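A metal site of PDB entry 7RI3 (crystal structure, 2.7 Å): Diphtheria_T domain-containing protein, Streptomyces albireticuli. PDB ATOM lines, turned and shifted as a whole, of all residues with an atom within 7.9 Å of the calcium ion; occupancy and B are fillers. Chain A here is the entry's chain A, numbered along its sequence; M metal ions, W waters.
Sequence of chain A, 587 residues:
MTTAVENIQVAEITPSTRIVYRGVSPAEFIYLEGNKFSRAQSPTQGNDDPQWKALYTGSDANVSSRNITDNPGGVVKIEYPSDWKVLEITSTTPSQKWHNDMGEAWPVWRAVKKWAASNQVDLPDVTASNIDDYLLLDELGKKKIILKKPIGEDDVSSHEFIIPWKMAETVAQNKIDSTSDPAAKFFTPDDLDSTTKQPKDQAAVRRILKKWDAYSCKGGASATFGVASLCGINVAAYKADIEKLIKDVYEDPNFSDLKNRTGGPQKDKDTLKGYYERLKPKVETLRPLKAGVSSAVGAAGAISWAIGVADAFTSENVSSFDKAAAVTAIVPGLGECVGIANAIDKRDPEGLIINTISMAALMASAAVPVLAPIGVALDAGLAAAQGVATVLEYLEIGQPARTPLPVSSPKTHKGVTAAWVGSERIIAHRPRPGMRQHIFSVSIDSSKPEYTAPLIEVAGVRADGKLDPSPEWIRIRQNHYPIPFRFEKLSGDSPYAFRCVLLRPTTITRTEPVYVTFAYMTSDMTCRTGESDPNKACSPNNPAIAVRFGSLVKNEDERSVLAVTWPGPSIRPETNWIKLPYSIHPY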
ATOM      1  N   CYS A 217     -22.743 -20.760  -7.979  1.00  0.00           N
ATOM      2  CA  CYS A 217     -23.478 -21.953  -8.361  1.00  0.00           C
ATOM      3  C   CYS A 217     -24.544 -22.336  -7.347  1.00  0.00           C
ATOM      4  O   CYS A 217     -25.268 -23.319  -7.555  1.00  0.00           O
ATOM      5  CB  CYS A 217     -22.496 -23.109  -8.557  1.00  0.00           C
ATOM      6  SG  CYS A 217     -21.121 -22.675  -9.619  1.00  0.00           S
ATOM      7  N   SER A 229     -27.429 -27.687  -7.979  1.00  0.00           N
ATOM      8  CA  SER A 229     -26.432 -26.690  -8.350  1.00  0.00           C
ATOM      9  C   SER A 229     -26.685 -26.124  -9.753  1.00  0.00           C
ATOM     10  O   SER A 229     -27.094 -26.847 -10.660  1.00  0.00           O
ATOM     11  CB  SER A 229     -25.022 -27.293  -8.287  1.00  0.00           C
ATOM     12  OG  SER A 229     -24.054 -26.363  -8.748  1.00  0.00           O
ATOM     13  N   LEU A 230     -26.425 -24.824  -9.935  1.00  0.00           N
ATOM     14  CA  LEU A 230     -26.637 -24.218 -11.246  1.00  0.00           C
ATOM     15  C   LEU A 230     -25.520 -24.562 -12.225  1.00  0.00           C
ATOM     16  O   LEU A 230     -25.744 -24.526 -13.446  1.00  0.00           O
ATOM     17  CB  LEU A 230     -26.736 -22.706 -11.122  1.00  0.00           C
ATOM     18  CG  LEU A 230     -27.948 -22.144 -10.390  1.00  0.00           C
ATOM     19  CD1 LEU A 230     -27.737 -20.663 -10.218  1.00  0.00           C
ATOM     20  CD2 LEU A 230     -29.223 -22.429 -11.170  1.00  0.00           C
ATOM     21  N   CYS A 231     -24.332 -24.866 -11.732  1.00  0.00           N
ATOM     22  CA  CYS A 231     -23.174 -25.021 -12.597  1.00  0.00           C
ATOM     23  C   CYS A 231     -23.022 -26.433 -13.134  1.00  0.00           C
ATOM     24  O   CYS A 231     -22.300 -26.633 -14.119  1.00  0.00           O
ATOM     25  CB  CYS A 231     -21.914 -24.593 -11.854  1.00  0.00           C
ATOM     26  SG  CYS A 231     -21.905 -22.807 -11.488  1.00  0.00           S
ATOM     27  N   GLY A 232     -23.704 -27.399 -12.533  1.00  0.00           N
ATOM     28  CA  GLY A 232     -23.632 -28.765 -12.978  1.00  0.00           C
ATOM     29  C   GLY A 232     -22.708 -29.604 -12.131  1.00  0.00           C
ATOM     30  O   GLY A 232     -22.412 -29.278 -10.978  1.00  0.00           O
ATOM     31  N   ILE A 233     -22.220 -30.685 -12.738  1.00  0.00           N
ATOM     32  CA  ILE A 233     -21.365 -31.635 -12.035  1.00  0.00           C
ATOM     33  C   ILE A 233     -20.293 -30.889 -11.259  1.00  0.00           C
ATOM     34  O   ILE A 233     -19.682 -29.948 -11.764  1.00  0.00           O
ATOM     35  CB  ILE A 233     -20.736 -32.628 -13.012  1.00  0.00           C
ATOM     36  CG1 ILE A 233     -21.811 -33.353 -13.812  1.00  0.00           C
ATOM     37  CG2 ILE A 233     -19.860 -33.606 -12.258  1.00  0.00           C
ATOM     38  CD1 ILE A 233     -23.037 -33.693 -13.003  1.00  0.00           C
ATOM     39  N   ASN A 234     -20.067 -31.305 -10.016  1.00  0.00           N
ATOM     40  CA  ASN A 234     -19.006 -30.744  -9.185  1.00  0.00           C
ATOM     41  C   ASN A 234     -17.792 -31.646  -9.311  1.00  0.00           C
ATOM     42  O   ASN A 234     -17.668 -32.643  -8.592  1.00  0.00           O
ATOM     43  CB  ASN A 234     -19.454 -30.613  -7.738  1.00  0.00           C
ATOM     44  CG  ASN A 234     -18.558 -29.696  -6.933  1.00  0.00           C
ATOM     45  OD1 ASN A 234     -17.479 -29.310  -7.394  1.00  0.00           O
ATOM     46  ND2 ASN A 234     -19.004 -29.334  -5.735  1.00  0.00           N
ATOM     47  N   VAL A 235     -16.884 -31.302 -10.233  1.00  0.00           N
ATOM     48  CA  VAL A 235     -15.725 -32.142 -10.499  1.00  0.00           C
ATOM     49  C   VAL A 235     -14.901 -32.313  -9.238  1.00  0.00           C
ATOM     50  O   VAL A 235     -14.312 -33.374  -9.004  1.00  0.00           O
ATOM     51  CB  VAL A 235     -14.874 -31.550 -11.635  1.00  0.00           C
ATOM     52  CG1 VAL A 235     -13.692 -32.436 -11.917  1.00  0.00           C
ATOM     53  CG2 VAL A 235     -15.722 -31.378 -12.879  1.00  0.00           C
ATOM     54  N   ALA A 236     -14.845 -31.279  -8.397  1.00  0.00           N
ATOM     55  CA  ALA A 236     -14.050 -31.365  -7.185  1.00  0.00           C
ATOM     56  C   ALA A 236     -14.508 -32.523  -6.311  1.00  0.00           C
ATOM     57  O   ALA A 236     -13.718 -33.057  -5.528  1.00  0.00           O
ATOM     58  CB  ALA A 236     -14.124 -30.045  -6.420  1.00  0.00           C
ATOM     59  N   ALA A 389      -8.825 -31.595 -13.884  1.00  0.00           N
ATOM     60  CA  ALA A 389     -10.072 -31.399 -13.137  1.00  0.00           C
ATOM     61  C   ALA A 389     -10.467 -29.933 -13.104  1.00  0.00           C
ATOM     62  O   ALA A 389     -11.640 -29.594 -13.239  1.00  0.00           O
ATOM     63  CB  ALA A 389      -9.932 -31.954 -11.722  1.00  0.00           C
ATOM     64  N   THR A 390      -9.485 -29.030 -12.937  1.00  0.00           N
ATOM     65  CA  THR A 390      -9.799 -27.614 -12.960  1.00  0.00           C
ATOM     66  C   THR A 390     -10.462 -27.206 -14.274  1.00  0.00           C
ATOM     67  O   THR A 390     -11.425 -26.436 -14.283  1.00  0.00           O
ATOM     68  CB  THR A 390      -8.528 -26.799 -12.698  1.00  0.00           C
ATOM     69  OG1 THR A 390      -8.046 -27.082 -11.378  1.00  0.00           O
ATOM     70  CG2 THR A 390      -8.813 -25.301 -12.810  1.00  0.00           C
ATOM     71  N   VAL A 391      -9.976 -27.734 -15.398  1.00  0.00           N
ATOM     72  CA  VAL A 391     -10.551 -27.365 -16.686  1.00  0.00           C
ATOM     73  C   VAL A 391     -12.017 -27.800 -16.753  1.00  0.00           C
ATOM     74  O   VAL A 391     -12.921 -26.997 -16.980  1.00  0.00           O
ATOM     75  CB  VAL A 391      -9.727 -27.959 -17.841  1.00  0.00           C
ATOM     76  CG1 VAL A 391     -10.495 -27.842 -19.157  1.00  0.00           C
ATOM     77  CG2 VAL A 391      -8.395 -27.258 -17.941  1.00  0.00           C
ATOM     78  N   LEU A 392     -12.261 -29.100 -16.528  1.00  0.00           N
ATOM     79  CA  LEU A 392     -13.614 -29.639 -16.651  1.00  0.00           C
ATOM     80  C   LEU A 392     -14.566 -29.020 -15.652  1.00  0.00           C
ATOM     81  O   LEU A 392     -15.780 -28.964 -15.891  1.00  0.00           O
ATOM     82  CB  LEU A 392     -13.573 -31.155 -16.487  1.00  0.00           C
ATOM     83  CG  LEU A 392     -12.737 -31.829 -17.564  1.00  0.00           C
ATOM     84  CD1 LEU A 392     -12.638 -33.304 -17.265  1.00  0.00           C
ATOM     85  CD2 LEU A 392     -13.343 -31.572 -18.940  1.00  0.00           C
ATOM     86  N   GLU A 393     -14.047 -28.575 -14.503  1.00  0.00           N
ATOM     87  CA  GLU A 393     -14.910 -28.031 -13.473  1.00  0.00           C
ATOM     88  C   GLU A 393     -15.721 -26.849 -13.971  1.00  0.00           C
ATOM     89  O   GLU A 393     -16.874 -26.674 -13.564  1.00  0.00           O
ATOM     90  CB  GLU A 393     -14.062 -27.604 -12.266  1.00  0.00           C
ATOM     91  CG  GLU A 393     -14.861 -27.047 -11.124  1.00  0.00           C
ATOM     92  CD  GLU A 393     -15.745 -28.088 -10.477  1.00  0.00           C
ATOM     93  OE1 GLU A 393     -16.850 -28.335 -11.009  1.00  0.00           O
ATOM     94  OE2 GLU A 393     -15.326 -28.661  -9.452  1.00  0.00           O
ATOM     95  N   TYR A 394     -15.139 -26.051 -14.863  1.00  0.00           N
ATOM     96  CA  TYR A 394     -15.723 -24.807 -15.337  1.00  0.00           C
ATOM     97  C   TYR A 394     -16.545 -24.978 -16.618  1.00  0.00           C
ATOM     98  O   TYR A 394     -17.074 -23.984 -17.131  1.00  0.00           O
ATOM     99  CB  TYR A 394     -14.614 -23.776 -15.547  1.00  0.00           C
ATOM    100  CG  TYR A 394     -14.031 -23.267 -14.240  1.00  0.00           C
ATOM    101  CD1 TYR A 394     -14.813 -22.525 -13.356  1.00  0.00           C
ATOM    102  CD2 TYR A 394     -12.711 -23.523 -13.896  1.00  0.00           C
ATOM    103  CE1 TYR A 394     -14.288 -22.051 -12.167  1.00  0.00           C
ATOM    104  CE2 TYR A 394     -12.179 -23.050 -12.713  1.00  0.00           C
ATOM    105  CZ  TYR A 394     -12.975 -22.316 -11.851  1.00  0.00           C
ATOM    106  OH  TYR A 394     -12.456 -21.838 -10.669  1.00  0.00           O
ATOM    107  N   LEU A 395     -16.675 -26.197 -17.124  1.00  0.00           N
ATOM    108  CA  LEU A 395     -17.568 -26.503 -18.229  1.00  0.00           C
ATOM    109  C   LEU A 395     -18.854 -27.088 -17.662  1.00  0.00           C
ATOM    110  O   LEU A 395     -18.819 -27.842 -16.687  1.00  0.00           O
ATOM    111  CB  LEU A 395     -16.931 -27.461 -19.217  1.00  0.00           C
ATOM    112  CG  LEU A 395     -15.623 -26.949 -19.815  1.00  0.00           C
ATOM    113  CD1 LEU A 395     -14.979 -27.985 -20.695  1.00  0.00           C
ATOM    114  CD2 LEU A 395     -15.870 -25.657 -20.582  1.00  0.00           C
ATOM    115  N   GLU A 396     -19.984 -26.735 -18.270  1.00  0.00           N
ATOM    116  CA  GLU A 396     -21.271 -27.297 -17.848  1.00  0.00           C
ATOM    117  C   GLU A 396     -21.521 -28.562 -18.651  1.00  0.00           C
ATOM    118  O   GLU A 396     -22.329 -28.604 -19.585  1.00  0.00           O
ATOM    119  CB  GLU A 396     -22.385 -26.281 -18.012  1.00  0.00           C
ATOM    120  CG  GLU A 396     -22.255 -25.114 -17.057  1.00  0.00           C
ATOM    121  CD  GLU A 396     -23.419 -24.142 -17.095  1.00  0.00           C
ATOM    122  OE1 GLU A 396     -24.398 -24.365 -17.854  1.00  0.00           O
ATOM    123  OE2 GLU A 396     -23.337 -23.121 -16.358  1.00  0.00           O
ATOM    124  N   ILE A 397     -20.796 -29.613 -18.272  1.00  0.00           N
ATOM    125  CA  ILE A 397     -21.003 -30.937 -18.846  1.00  0.00           C
ATOM    126  C   ILE A 397     -22.255 -31.532 -18.227  1.00  0.00           C
ATOM    127  O   ILE A 397     -22.559 -31.302 -17.040  1.00  0.00           O
ATOM    128  CB  ILE A 397     -19.776 -31.840 -18.580  1.00  0.00           C
ATOM    129  CG1 ILE A 397     -18.480 -31.096 -18.844  1.00  0.00           C
ATOM    130  CG2 ILE A 397     -19.819 -33.067 -19.454  1.00  0.00           C
ATOM    131  CD1 ILE A 397     -17.268 -31.845 -18.382  1.00  0.00           C
ATOM    132  N   ASN A 479     -20.949 -19.504 -19.108  1.00  0.00           N
ATOM    133  CA  ASN A 479     -22.036 -20.213 -18.451  1.00  0.00           C
ATOM    134  C   ASN A 479     -22.296 -19.569 -17.095  1.00  0.00           C
ATOM    135  O   ASN A 479     -22.086 -18.357 -16.951  1.00  0.00           O
ATOM    136  CB  ASN A 479     -21.693 -21.708 -18.308  1.00  0.00           C
ATOM    137  CG  ASN A 479     -20.272 -21.938 -17.854  1.00  0.00           C
ATOM    138  OD1 ASN A 479     -19.717 -21.150 -17.094  1.00  0.00           O
ATOM    139  ND2 ASN A 479     -19.673 -23.034 -18.314  1.00  0.00           N
ATOM    140  N   TYR A 481     -20.640 -19.891 -14.313  1.00  0.00           N
ATOM    141  CA  TYR A 481     -19.450 -19.504 -13.578  1.00  0.00           C
ATOM    142  C   TYR A 481     -19.018 -18.082 -13.929  1.00  0.00           C
ATOM    143  O   TYR A 481     -19.168 -17.649 -15.079  1.00  0.00           O
ATOM    144  CB  TYR A 481     -18.290 -20.439 -13.888  1.00  0.00           C
ATOM    145  CG  TYR A 481     -18.283 -21.752 -13.152  1.00  0.00           C
ATOM    146  CD1 TYR A 481     -17.988 -21.793 -11.807  1.00  0.00           C
ATOM    147  CD2 TYR A 481     -18.541 -22.960 -13.810  1.00  0.00           C
ATOM    148  CE1 TYR A 481     -17.973 -22.987 -11.124  1.00  0.00           C
ATOM    149  CE2 TYR A 481     -18.518 -24.155 -13.133  1.00  0.00           C
ATOM    150  CZ  TYR A 481     -18.234 -24.168 -11.790  1.00  0.00           C
ATOM    151  OH  TYR A 481     -18.199 -25.336 -11.078  1.00  0.00           O
HETATM  152 CA    CA M   1     -18.665 -27.855 -12.313  1.00  0.00          CA
HETATM  153  O   HOH W   1     -20.220 -26.801  -9.997  1.00  0.00           O
HETATM  154  O   HOH W   2     -19.833 -27.390 -14.322  1.00  0.00           O
HETATM  155  O   HOH W   3     -18.010 -29.487 -14.173  1.00  0.00           O
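Three residues have an atom within 4 Å of the calcium ion: Ile 233, Glu 393 and Tyr 481.
The nearest printed residue that does not touch the calcium ion is Gly 232 (4.2 Å).
OD1 of Asn 234 sits close to OE2 of Glu 393, at 3.0 Å.
The backbone NH (N) of Val 235 is in hydrogen-bond range of the side-chain carboxylate (OE2) of Glu 393.
The side-chain carboxylate (OE2) of Glu 393 lies within hydrogen-bond range of the backbone NH (N) of Ala 236, at 2.9 Å.
N of Tyr 481 sits at hydrogen-bond distance from OD1 of Asn 479.
The side-chain sulfur (SG) of Cys 231 forms a disulfide with the side-chain sulfur (SG) of Cys 217, 2.0 Å away.
Water W2 lies within hydrogen-bond range of O of Cys 231 (2.6 Å) and O of Leu 395 (2.6 Å).
OE1 of Glu 393 binds the calcium ion, 2.3 Å away.
The calcium ion is bound by water W2 (2.4 Å).
O of Ile 233 is bound to the calcium ion (2.4 Å).
O of Glu 393 binds the calcium ion (2.5 Å).
Water W3 binds the calcium ion, 2.6 Å away.
The side-chain hydroxyl (OH) of Tyr 481 is bound to the calcium ion, at 2.8 Å.
The calcium ion has six donor atoms within binding distance.
Slightly farther from the calcium ion lies water W1 (3.0 Å).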
